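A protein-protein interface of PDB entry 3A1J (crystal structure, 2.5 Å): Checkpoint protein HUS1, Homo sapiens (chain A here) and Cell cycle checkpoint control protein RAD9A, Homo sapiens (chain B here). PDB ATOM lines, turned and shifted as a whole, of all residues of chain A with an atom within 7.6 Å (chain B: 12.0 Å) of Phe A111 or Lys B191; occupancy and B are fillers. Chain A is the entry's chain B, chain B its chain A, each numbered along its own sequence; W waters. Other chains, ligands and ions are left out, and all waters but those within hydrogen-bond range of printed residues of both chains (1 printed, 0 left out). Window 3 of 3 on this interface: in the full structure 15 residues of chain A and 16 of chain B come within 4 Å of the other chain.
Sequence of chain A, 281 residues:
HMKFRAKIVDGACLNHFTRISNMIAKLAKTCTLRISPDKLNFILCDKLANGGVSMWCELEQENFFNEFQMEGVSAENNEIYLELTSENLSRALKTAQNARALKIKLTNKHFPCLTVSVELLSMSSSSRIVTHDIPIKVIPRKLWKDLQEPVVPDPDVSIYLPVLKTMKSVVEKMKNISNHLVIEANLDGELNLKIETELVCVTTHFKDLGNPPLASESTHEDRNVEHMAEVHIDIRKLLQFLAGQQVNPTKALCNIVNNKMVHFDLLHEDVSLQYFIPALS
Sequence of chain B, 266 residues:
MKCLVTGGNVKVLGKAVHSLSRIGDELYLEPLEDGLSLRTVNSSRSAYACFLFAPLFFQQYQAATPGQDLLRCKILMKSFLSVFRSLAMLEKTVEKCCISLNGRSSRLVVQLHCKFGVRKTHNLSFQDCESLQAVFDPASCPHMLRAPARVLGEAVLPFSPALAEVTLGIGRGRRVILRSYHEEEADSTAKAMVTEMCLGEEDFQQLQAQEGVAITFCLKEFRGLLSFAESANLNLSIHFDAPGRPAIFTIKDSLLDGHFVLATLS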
ATOM      1  N   THR A  85     -28.430   9.146  31.508  1.00  0.00           N
ATOM      2  CA  THR A  85     -27.923   9.385  32.857  1.00  0.00           C
ATOM      3  C   THR A  85     -29.148   9.824  33.662  1.00  0.00           C
ATOM      4  O   THR A  85     -29.781  10.836  33.364  1.00  0.00           O
ATOM      5  CB  THR A  85     -26.860  10.509  32.898  1.00  0.00           C
ATOM      6  OG1 THR A  85     -25.720  10.132  32.119  1.00  0.00           O
ATOM      7  CG2 THR A  85     -26.399  10.751  34.327  1.00  0.00           C
ATOM      8  N   ASN A  88     -29.857  13.305  35.018  1.00  0.00           N
ATOM      9  CA  ASN A  88     -30.198  14.194  33.926  1.00  0.00           C
ATOM     10  C   ASN A  88     -31.716  14.395  33.862  1.00  0.00           C
ATOM     11  O   ASN A  88     -32.199  15.522  33.777  1.00  0.00           O
ATOM     12  CB  ASN A  88     -29.669  13.620  32.605  1.00  0.00           C
ATOM     13  CG  ASN A  88     -28.205  13.963  32.361  1.00  0.00           C
ATOM     14  OD1 ASN A  88     -27.485  14.326  33.280  1.00  0.00           O
ATOM     15  ND2 ASN A  88     -27.764  13.839  31.117  1.00  0.00           N
ATOM     16  N   LEU A 106     -38.225  12.936  21.556  1.00  0.00           N
ATOM     17  CA  LEU A 106     -36.931  12.459  21.077  1.00  0.00           C
ATOM     18  C   LEU A 106     -36.515  13.384  19.929  1.00  0.00           C
ATOM     19  O   LEU A 106     -37.234  13.516  18.939  1.00  0.00           O
ATOM     20  CB  LEU A 106     -37.054  11.019  20.581  1.00  0.00           C
ATOM     21  CG  LEU A 106     -35.836  10.361  19.939  1.00  0.00           C
ATOM     22  CD1 LEU A 106     -34.712  10.254  20.948  1.00  0.00           C
ATOM     23  CD2 LEU A 106     -36.224   8.981  19.430  1.00  0.00           C
ATOM     24  N   THR A 107     -35.364  14.033  20.069  1.00  0.00           N
ATOM     25  CA  THR A 107     -34.891  14.953  19.045  1.00  0.00           C
ATOM     26  C   THR A 107     -33.477  14.602  18.605  1.00  0.00           C
ATOM     27  O   THR A 107     -32.870  13.670  19.130  1.00  0.00           O
ATOM     28  CB  THR A 107     -34.903  16.413  19.560  1.00  0.00           C
ATOM     29  OG1 THR A 107     -34.026  16.535  20.688  1.00  0.00           O
ATOM     30  CG2 THR A 107     -36.303  16.824  19.972  1.00  0.00           C
ATOM     31  N   ASN A 108     -32.956  15.357  17.642  1.00  0.00           N
ATOM     32  CA  ASN A 108     -31.611  15.126  17.130  1.00  0.00           C
ATOM     33  C   ASN A 108     -30.988  16.410  16.588  1.00  0.00           C
ATOM     34  O   ASN A 108     -30.471  16.429  15.472  1.00  0.00           O
ATOM     35  CB  ASN A 108     -31.645  14.080  16.015  1.00  0.00           C
ATOM     36  CG  ASN A 108     -30.289  13.445  15.773  1.00  0.00           C
ATOM     37  OD1 ASN A 108     -29.243  14.100  15.891  1.00  0.00           O
ATOM     38  ND2 ASN A 108     -30.297  12.164  15.424  1.00  0.00           N
ATOM     39  N   LYS A 109     -31.033  17.480  17.376  1.00  0.00           N
ATOM     40  CA  LYS A 109     -30.472  18.767  16.961  1.00  0.00           C
ATOM     41  C   LYS A 109     -28.960  18.650  16.770  1.00  0.00           C
ATOM     42  O   LYS A 109     -28.485  18.555  15.643  1.00  0.00           O
ATOM     43  CB  LYS A 109     -30.798  19.843  18.005  1.00  0.00           C
ATOM     44  CG  LYS A 109     -32.295  19.972  18.307  1.00  0.00           C
ATOM     45  CD  LYS A 109     -32.557  20.855  19.520  1.00  0.00           C
ATOM     46  CE  LYS A 109     -33.974  20.673  20.044  1.00  0.00           C
ATOM     47  NZ  LYS A 109     -34.202  21.428  21.312  1.00  0.00           N
ATOM     48  N   HIS A 110     -28.213  18.656  17.872  1.00  0.00           N
ATOM     49  CA  HIS A 110     -26.763  18.526  17.806  1.00  0.00           C
ATOM     50  C   HIS A 110     -26.392  17.053  17.796  1.00  0.00           C
ATOM     51  O   HIS A 110     -25.341  16.665  17.298  1.00  0.00           O
ATOM     52  CB  HIS A 110     -26.113  19.195  19.013  1.00  0.00           C
ATOM     53  CG  HIS A 110     -26.136  20.690  18.964  1.00  0.00           C
ATOM     54  ND1 HIS A 110     -27.306  21.416  18.930  1.00  0.00           N
ATOM     55  CD2 HIS A 110     -25.130  21.596  18.936  1.00  0.00           C
ATOM     56  CE1 HIS A 110     -27.020  22.706  18.883  1.00  0.00           C
ATOM     57  NE2 HIS A 110     -25.705  22.842  18.886  1.00  0.00           N
ATOM     58  N   PHE A 111     -27.276  16.241  18.362  1.00  0.00           N
ATOM     59  CA  PHE A 111     -27.096  14.798  18.455  1.00  0.00           C
ATOM     60  C   PHE A 111     -28.301  14.266  19.213  1.00  0.00           C
ATOM     61  O   PHE A 111     -29.002  15.030  19.874  1.00  0.00           O
ATOM     62  CB  PHE A 111     -25.814  14.454  19.219  1.00  0.00           C
ATOM     63  CG  PHE A 111     -25.650  15.216  20.503  1.00  0.00           C
ATOM     64  CD1 PHE A 111     -24.790  16.309  20.572  1.00  0.00           C
ATOM     65  CD2 PHE A 111     -26.369  14.857  21.641  1.00  0.00           C
ATOM     66  CE1 PHE A 111     -24.650  17.034  21.760  1.00  0.00           C
ATOM     67  CE2 PHE A 111     -26.233  15.576  22.827  1.00  0.00           C
ATOM     68  CZ  PHE A 111     -25.376  16.664  22.886  1.00  0.00           C
ATOM     69  N   PRO A 112     -28.556  12.951  19.135  1.00  0.00           N
ATOM     70  CA  PRO A 112     -29.705  12.377  19.838  1.00  0.00           C
ATOM     71  C   PRO A 112     -29.858  12.768  21.310  1.00  0.00           C
ATOM     72  O   PRO A 112     -28.949  12.612  22.124  1.00  0.00           O
ATOM     73  CB  PRO A 112     -29.536  10.868  19.621  1.00  0.00           C
ATOM     74  CG  PRO A 112     -28.078  10.702  19.322  1.00  0.00           C
ATOM     75  CD  PRO A 112     -27.783  11.897  18.460  1.00  0.00           C
ATOM     76  N   CYS A 113     -31.038  13.292  21.621  1.00  0.00           N
ATOM     77  CA  CYS A 113     -31.401  13.731  22.958  1.00  0.00           C
ATOM     78  C   CYS A 113     -32.872  13.488  23.219  1.00  0.00           C
ATOM     79  O   CYS A 113     -33.682  13.336  22.302  1.00  0.00           O
ATOM     80  CB  CYS A 113     -31.189  15.236  23.127  1.00  0.00           C
ATOM     81  SG  CYS A 113     -29.516  15.804  23.137  1.00  0.00           S
ATOM     82  N   LEU A 114     -33.213  13.459  24.492  1.00  0.00           N
ATOM     83  CA  LEU A 114     -34.596  13.341  24.868  1.00  0.00           C
ATOM     84  C   LEU A 114     -34.742  14.786  25.343  1.00  0.00           C
ATOM     85  O   LEU A 114     -34.077  15.193  26.293  1.00  0.00           O
ATOM     86  CB  LEU A 114     -34.751  12.341  26.008  1.00  0.00           C
ATOM     87  CG  LEU A 114     -36.135  11.736  26.239  1.00  0.00           C
ATOM     88  CD1 LEU A 114     -36.626  11.001  24.999  1.00  0.00           C
ATOM     89  CD2 LEU A 114     -36.050  10.777  27.413  1.00  0.00           C
ATOM     90  N   THR A 115     -35.541  15.581  24.639  1.00  0.00           N
ATOM     91  CA  THR A 115     -35.725  16.974  25.012  1.00  0.00           C
ATOM     92  C   THR A 115     -36.969  17.135  25.876  1.00  0.00           C
ATOM     93  O   THR A 115     -38.067  16.751  25.476  1.00  0.00           O
ATOM     94  CB  THR A 115     -35.846  17.879  23.758  1.00  0.00           C
ATOM     95  OG1 THR A 115     -34.600  17.886  23.052  1.00  0.00           O
ATOM     96  CG2 THR A 115     -36.180  19.309  24.153  1.00  0.00           C
ATOM     97  N   ASP A 133     -31.973  19.428  26.986  1.00  0.00           N
ATOM     98  CA  ASP A 133     -31.640  18.458  25.956  1.00  0.00           C
ATOM     99  C   ASP A 133     -30.811  17.357  26.590  1.00  0.00           C
ATOM    100  O   ASP A 133     -29.613  17.514  26.842  1.00  0.00           O
ATOM    101  CB  ASP A 133     -30.897  19.134  24.808  1.00  0.00           C
ATOM    102  CG  ASP A 133     -31.771  20.127  24.075  1.00  0.00           C
ATOM    103  OD1 ASP A 133     -32.853  19.721  23.607  1.00  0.00           O
ATOM    104  OD2 ASP A 133     -31.393  21.311  23.968  1.00  0.00           O
ATOM    105  N   ILE A 134     -31.473  16.244  26.867  1.00  0.00           N
ATOM    106  CA  ILE A 134     -30.837  15.112  27.514  1.00  0.00           C
ATOM    107  C   ILE A 134     -30.169  14.166  26.532  1.00  0.00           C
ATOM    108  O   ILE A 134     -30.836  13.536  25.712  1.00  0.00           O
ATOM    109  CB  ILE A 134     -31.865  14.310  28.337  1.00  0.00           C
ATOM    110  CG1 ILE A 134     -32.706  15.270  29.196  1.00  0.00           C
ATOM    111  CG2 ILE A 134     -31.156  13.279  29.173  1.00  0.00           C
ATOM    112  CD1 ILE A 134     -33.573  14.595  30.252  1.00  0.00           C
ATOM    113  N   PRO A 135     -28.839  14.057  26.603  1.00  0.00           N
ATOM    114  CA  PRO A 135     -28.111  13.161  25.701  1.00  0.00           C
ATOM    115  C   PRO A 135     -28.516  11.696  25.936  1.00  0.00           C
ATOM    116  O   PRO A 135     -28.479  11.207  27.067  1.00  0.00           O
ATOM    117  CB  PRO A 135     -26.644  13.402  26.079  1.00  0.00           C
ATOM    118  CG  PRO A 135     -26.642  14.785  26.646  1.00  0.00           C
ATOM    119  CD  PRO A 135     -27.909  14.820  27.455  1.00  0.00           C
ATOM    120  N   ILE A 136     -28.916  11.004  24.874  1.00  0.00           N
ATOM    121  CA  ILE A 136     -29.281   9.598  24.987  1.00  0.00           C
ATOM    122  C   ILE A 136     -28.536   8.797  23.941  1.00  0.00           C
ATOM    123  O   ILE A 136     -28.095   9.335  22.930  1.00  0.00           O
ATOM    124  CB  ILE A 136     -30.781   9.349  24.756  1.00  0.00           C
ATOM    125  CG1 ILE A 136     -31.193   9.929  23.402  1.00  0.00           C
ATOM    126  CG2 ILE A 136     -31.590   9.949  25.889  1.00  0.00           C
ATOM    127  CD1 ILE A 136     -31.863   8.923  22.483  1.00  0.00           C
ATOM    128  N   LEU B 163     -23.055  25.234  37.819  1.00  0.00           N
ATOM    129  CA  LEU B 163     -22.813  25.736  36.464  1.00  0.00           C
ATOM    130  C   LEU B 163     -21.854  26.924  36.505  1.00  0.00           C
ATOM    131  O   LEU B 163     -22.078  27.887  37.237  1.00  0.00           O
ATOM    132  CB  LEU B 163     -24.129  26.173  35.806  1.00  0.00           C
ATOM    133  CG  LEU B 163     -24.000  26.746  34.389  1.00  0.00           C
ATOM    134  CD1 LEU B 163     -23.283  25.736  33.476  1.00  0.00           C
ATOM    135  CD2 LEU B 163     -25.391  27.088  33.853  1.00  0.00           C
ATOM    136  N   ARG B 179     -28.974  30.383  28.755  1.00  0.00           N
ATOM    137  CA  ARG B 179     -28.592  29.045  28.330  1.00  0.00           C
ATOM    138  C   ARG B 179     -27.282  28.617  28.975  1.00  0.00           C
ATOM    139  O   ARG B 179     -26.346  29.415  29.091  1.00  0.00           O
ATOM    140  CB  ARG B 179     -28.462  29.005  26.797  1.00  0.00           C
ATOM    141  CG  ARG B 179     -28.279  27.612  26.219  1.00  0.00           C
ATOM    142  CD  ARG B 179     -28.041  27.604  24.699  1.00  0.00           C
ATOM    143  NE  ARG B 179     -29.198  28.047  23.919  1.00  0.00           N
ATOM    144  CZ  ARG B 179     -29.350  29.274  23.417  1.00  0.00           C
ATOM    145  NH1 ARG B 179     -28.413  30.200  23.610  1.00  0.00           N
ATOM    146  NH2 ARG B 179     -30.439  29.579  22.720  1.00  0.00           N
ATOM    147  N   SER B 180     -27.217  27.359  29.404  1.00  0.00           N
ATOM    148  CA  SER B 180     -25.998  26.859  30.020  1.00  0.00           C
ATOM    149  C   SER B 180     -24.910  26.790  28.952  1.00  0.00           C
ATOM    150  O   SER B 180     -25.183  26.461  27.796  1.00  0.00           O
ATOM    151  CB  SER B 180     -26.239  25.482  30.631  1.00  0.00           C
ATOM    152  OG  SER B 180     -26.870  24.613  29.708  1.00  0.00           O
ATOM    153  N   TYR B 181     -23.679  27.104  29.341  1.00  0.00           N
ATOM    154  CA  TYR B 181     -22.553  27.089  28.412  1.00  0.00           C
ATOM    155  C   TYR B 181     -21.452  26.137  28.875  1.00  0.00           C
ATOM    156  O   TYR B 181     -21.196  25.998  30.076  1.00  0.00           O
ATOM    157  CB  TYR B 181     -21.984  28.504  28.282  1.00  0.00           C
ATOM    158  CG  TYR B 181     -20.695  28.599  27.493  1.00  0.00           C
ATOM    159  CD1 TYR B 181     -20.703  28.925  26.135  1.00  0.00           C
ATOM    160  CD2 TYR B 181     -19.459  28.401  28.116  1.00  0.00           C
ATOM    161  CE1 TYR B 181     -19.519  29.059  25.422  1.00  0.00           C
ATOM    162  CE2 TYR B 181     -18.269  28.530  27.414  1.00  0.00           C
ATOM    163  CZ  TYR B 181     -18.303  28.863  26.065  1.00  0.00           C
ATOM    164  OH  TYR B 181     -17.118  29.018  25.373  1.00  0.00           O
ATOM    165  N   HIS B 182     -20.797  25.494  27.913  1.00  0.00           N
ATOM    166  CA  HIS B 182     -19.706  24.564  28.202  1.00  0.00           C
ATOM    167  C   HIS B 182     -18.680  24.602  27.080  1.00  0.00           C
ATOM    168  O   HIS B 182     -18.907  25.233  26.050  1.00  0.00           O
ATOM    169  CB  HIS B 182     -20.247  23.141  28.349  1.00  0.00           C
ATOM    170  CG  HIS B 182     -21.090  22.941  29.570  1.00  0.00           C
ATOM    171  ND1 HIS B 182     -20.551  22.792  30.832  1.00  0.00           N
ATOM    172  CD2 HIS B 182     -22.433  22.906  29.729  1.00  0.00           C
ATOM    173  CE1 HIS B 182     -21.528  22.674  31.714  1.00  0.00           C
ATOM    174  NE2 HIS B 182     -22.679  22.740  31.070  1.00  0.00           N
ATOM    175  N   GLU B 183     -17.551  23.933  27.279  1.00  0.00           N
ATOM    176  CA  GLU B 183     -16.508  23.886  26.258  1.00  0.00           C
ATOM    177  C   GLU B 183     -16.471  22.520  25.582  1.00  0.00           C
ATOM    178  O   GLU B 183     -17.506  21.890  25.360  1.00  0.00           O
ATOM    179  CB  GLU B 183     -15.137  24.156  26.870  1.00  0.00           C
ATOM    180  CG  GLU B 183     -14.885  25.577  27.314  1.00  0.00           C
ATOM    181  CD  GLU B 183     -13.515  25.727  27.964  1.00  0.00           C
ATOM    182  OE1 GLU B 183     -12.501  25.407  27.300  1.00  0.00           O
ATOM    183  OE2 GLU B 183     -13.454  26.157  29.141  1.00  0.00           O
ATOM    184  N   GLU B 184     -15.255  22.084  25.257  1.00  0.00           N
ATOM    185  CA  GLU B 184     -14.987  20.798  24.618  1.00  0.00           C
ATOM    186  C   GLU B 184     -16.046  20.403  23.592  1.00  0.00           C
ATOM    187  O   GLU B 184     -16.040  19.284  23.077  1.00  0.00           O
ATOM    188  CB  GLU B 184     -14.865  19.714  25.692  1.00  0.00           C
ATOM    189  CG  GLU B 184     -14.109  18.477  25.251  1.00  0.00           C
ATOM    190  CD  GLU B 184     -13.904  17.493  26.386  1.00  0.00           C
ATOM    191  OE1 GLU B 184     -13.399  17.914  27.450  1.00  0.00           O
ATOM    192  OE2 GLU B 184     -14.242  16.300  26.215  1.00  0.00           O
ATOM    193  N   ALA B 186     -14.580  19.251  20.862  1.00  0.00           N
ATOM    194  CA  ALA B 186     -14.068  17.886  20.802  1.00  0.00           C
ATOM    195  C   ALA B 186     -15.182  16.887  20.492  1.00  0.00           C
ATOM    196  O   ALA B 186     -16.190  16.832  21.198  1.00  0.00           O
ATOM    197  CB  ALA B 186     -13.389  17.525  22.120  1.00  0.00           C
ATOM    198  N   ASP B 187     -14.983  16.100  19.436  1.00  0.00           N
ATOM    199  CA  ASP B 187     -15.953  15.091  19.006  1.00  0.00           C
ATOM    200  C   ASP B 187     -15.892  13.881  19.946  1.00  0.00           C
ATOM    201  O   ASP B 187     -15.976  12.733  19.507  1.00  0.00           O
ATOM    202  CB  ASP B 187     -15.643  14.652  17.561  1.00  0.00           C
ATOM    203  CG  ASP B 187     -16.803  13.901  16.896  1.00  0.00           C
ATOM    204  OD1 ASP B 187     -17.285  12.892  17.457  1.00  0.00           O
ATOM    205  OD2 ASP B 187     -17.228  14.322  15.798  1.00  0.00           O
ATOM    206  N   SER B 188     -15.741  14.145  21.240  1.00  0.00           N
ATOM    207  CA  SER B 188     -15.667  13.076  22.231  1.00  0.00           C
ATOM    208  C   SER B 188     -17.021  12.844  22.903  1.00  0.00           C
ATOM    209  O   SER B 188     -17.964  13.620  22.719  1.00  0.00           O
ATOM    210  CB  SER B 188     -14.617  13.411  23.303  1.00  0.00           C
ATOM    211  OG  SER B 188     -14.983  14.556  24.058  1.00  0.00           O
ATOM    212  N   THR B 189     -17.111  11.765  23.674  1.00  0.00           N
ATOM    213  CA  THR B 189     -18.339  11.439  24.386  1.00  0.00           C
ATOM    214  C   THR B 189     -18.447  12.368  25.598  1.00  0.00           C
ATOM    215  O   THR B 189     -17.711  13.351  25.699  1.00  0.00           O
ATOM    216  CB  THR B 189     -18.342   9.948  24.848  1.00  0.00           C
ATOM    217  OG1 THR B 189     -19.551   9.668  25.569  1.00  0.00           O
ATOM    218  CG2 THR B 189     -17.128   9.647  25.732  1.00  0.00           C
ATOM    219  N   ALA B 190     -19.364  12.061  26.510  1.00  0.00           N
ATOM    220  CA  ALA B 190     -19.556  12.881  27.701  1.00  0.00           C
ATOM    221  C   ALA B 190     -20.089  14.259  27.327  1.00  0.00           C
ATOM    222  O   ALA B 190     -19.682  15.270  27.900  1.00  0.00           O
ATOM    223  CB  ALA B 190     -18.243  13.017  28.464  1.00  0.00           C
ATOM    224  N   LYS B 191     -20.993  14.296  26.355  1.00  0.00           N
ATOM    225  CA  LYS B 191     -21.591  15.554  25.924  1.00  0.00           C
ATOM    226  C   LYS B 191     -22.478  16.024  27.068  1.00  0.00           C
ATOM    227  O   LYS B 191     -23.213  15.232  27.658  1.00  0.00           O
ATOM    228  CB  LYS B 191     -22.432  15.334  24.667  1.00  0.00           C
ATOM    229  CG  LYS B 191     -21.690  14.596  23.558  1.00  0.00           C
ATOM    230  CD  LYS B 191     -22.656  13.794  22.700  1.00  0.00           C
ATOM    231  CE  LYS B 191     -21.908  12.888  21.732  1.00  0.00           C
ATOM    232  NZ  LYS B 191     -22.833  12.014  20.955  1.00  0.00           N
ATOM    233  N   ALA B 192     -22.408  17.310  27.384  1.00  0.00           N
ATOM    234  CA  ALA B 192     -23.196  17.862  28.475  1.00  0.00           C
ATOM    235  C   ALA B 192     -24.629  18.206  28.093  1.00  0.00           C
ATOM    236  O   ALA B 192     -24.912  18.569  26.947  1.00  0.00           O
ATOM    237  CB  ALA B 192     -22.505  19.102  29.038  1.00  0.00           C
ATOM    238  N   MET B 193     -25.524  18.079  29.072  1.00  0.00           N
ATOM    239  CA  MET B 193     -26.937  18.395  28.883  1.00  0.00           C
ATOM    240  C   MET B 193     -27.001  19.913  28.870  1.00  0.00           C
ATOM    241  O   MET B 193     -26.340  20.573  29.672  1.00  0.00           O
ATOM    242  CB  MET B 193     -27.789  17.835  30.052  1.00  0.00           C
ATOM    243  CG  MET B 193     -29.231  18.319  30.086  1.00  0.00           C
ATOM    244  SD  MET B 193     -30.176  17.672  31.721  1.00  0.00           S
ATOM    245  CE  MET B 193     -28.807  18.100  33.021  1.00  0.00           C
ATOM    246  N   VAL B 194     -27.775  20.468  27.944  1.00  0.00           N
ATOM    247  CA  VAL B 194     -27.891  21.908  27.891  1.00  0.00           C
ATOM    248  C   VAL B 194     -29.256  22.289  28.416  1.00  0.00           C
ATOM    249  O   VAL B 194     -30.246  21.601  28.168  1.00  0.00           O
ATOM    250  CB  VAL B 194     -27.705  22.475  26.455  1.00  0.00           C
ATOM    251  CG1 VAL B 194     -26.655  21.674  25.716  1.00  0.00           C
ATOM    252  CG2 VAL B 194     -29.019  22.504  25.718  1.00  0.00           C
ATOM    253  N   THR B 195     -29.291  23.378  29.168  1.00  0.00           N
ATOM    254  CA  THR B 195     -30.528  23.869  29.739  1.00  0.00           C
ATOM    255  C   THR B 195     -30.748  25.280  29.227  1.00  0.00           C
ATOM    256  O   THR B 195     -29.810  26.067  29.103  1.00  0.00           O
ATOM    257  CB  THR B 195     -30.465  23.903  31.279  1.00  0.00           C
ATOM    258  OG1 THR B 195     -30.282  22.576  31.783  1.00  0.00           O
ATOM    259  CG2 THR B 195     -31.753  24.492  31.850  1.00  0.00           C
HETATM  260  O   HOH W   1     -27.130  18.252  25.461  1.00  0.00           O
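NZ of Lys A109 is in salt-bridge range of OD1 of Asp A133, at 3.2 Å. The side-chain hydroxyl (OG1) of Thr A115 sits at hydrogen-bond distance from the side-chain carboxylate (OD1) of Asp A133, at 2.6 Å. The side-chain sulfur (SG) of Cys A113 lies close to the backbone carbonyl oxygen (O) of Phe A111, 3.4 Å away.
The side-chain sulfur (SD) of Met B193 lies close to the backbone carbonyl oxygen (O) of Asn A88, at 3.6 Å. The backbone carbonyl oxygen (O) of Val B194 is in hydrogen-bond range of the backbone NH (N) of Asp A133 (3.0 Å).
Among the printed residues, merely in contact across the chains: Asp A133 with Met B193, Pro A135 with Lys B191, Phe A111 with Lys B191 and Pro A135 with Met B193.
Water W1 lies within hydrogen-bond range of O of Ala B192 (2.7 Å), O of Asp A133 (2.9 Å) and N of Val B194 (3.4 Å).
Printed residues of chain A that touch a printed residue of chain B: Asn A88, Phe A111, Asp A133 and Pro A135. Hydrophobic or aromatic side chains of chain A that line the printed part of chain B: Phe A111 and Pro A135. Printed residues of chain B that touch a printed residue of chain A: Lys B191, Met B193 and Val B194. Hydrophobic or aromatic side chains of chain B within 4 Å of the printed part of chain A: Met B193 and Val B194. Among the printed residues, 6 pairs touch across the chains. Among the printed residues, no Asp or Glu carboxylate lies within 4 Å of a Lys or Arg side-chain nitrogen of the other chain.
Printed residues of chain B within 4 Å of Asn A88: Met B193. Thr A107 touches none of the printed residues of chain B. No residue of chain B comes within 4 Å of Asn A108. No residue of chain B comes within 4 Å of His A110. Of chain B, only Lys B191 (3.7 Å) comes within 4 Å of Phe A111. No residue of chain B comes within 4 Å of Cys A113. Leu A114 touches none of the printed residues of chain B. Of chain B, only Lys B191 and Met B193 come within 4 Å of Pro A135. Ala B186 touches none of the printed residues of chain A. Lys B191 touches two residues of chain A. Of the printed residues of chain A, Val B194 touches Asp A133 (3.0 Å). The nearest residue of chain A that does not touch Lys B191 is Pro A112 (5.5 Å).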
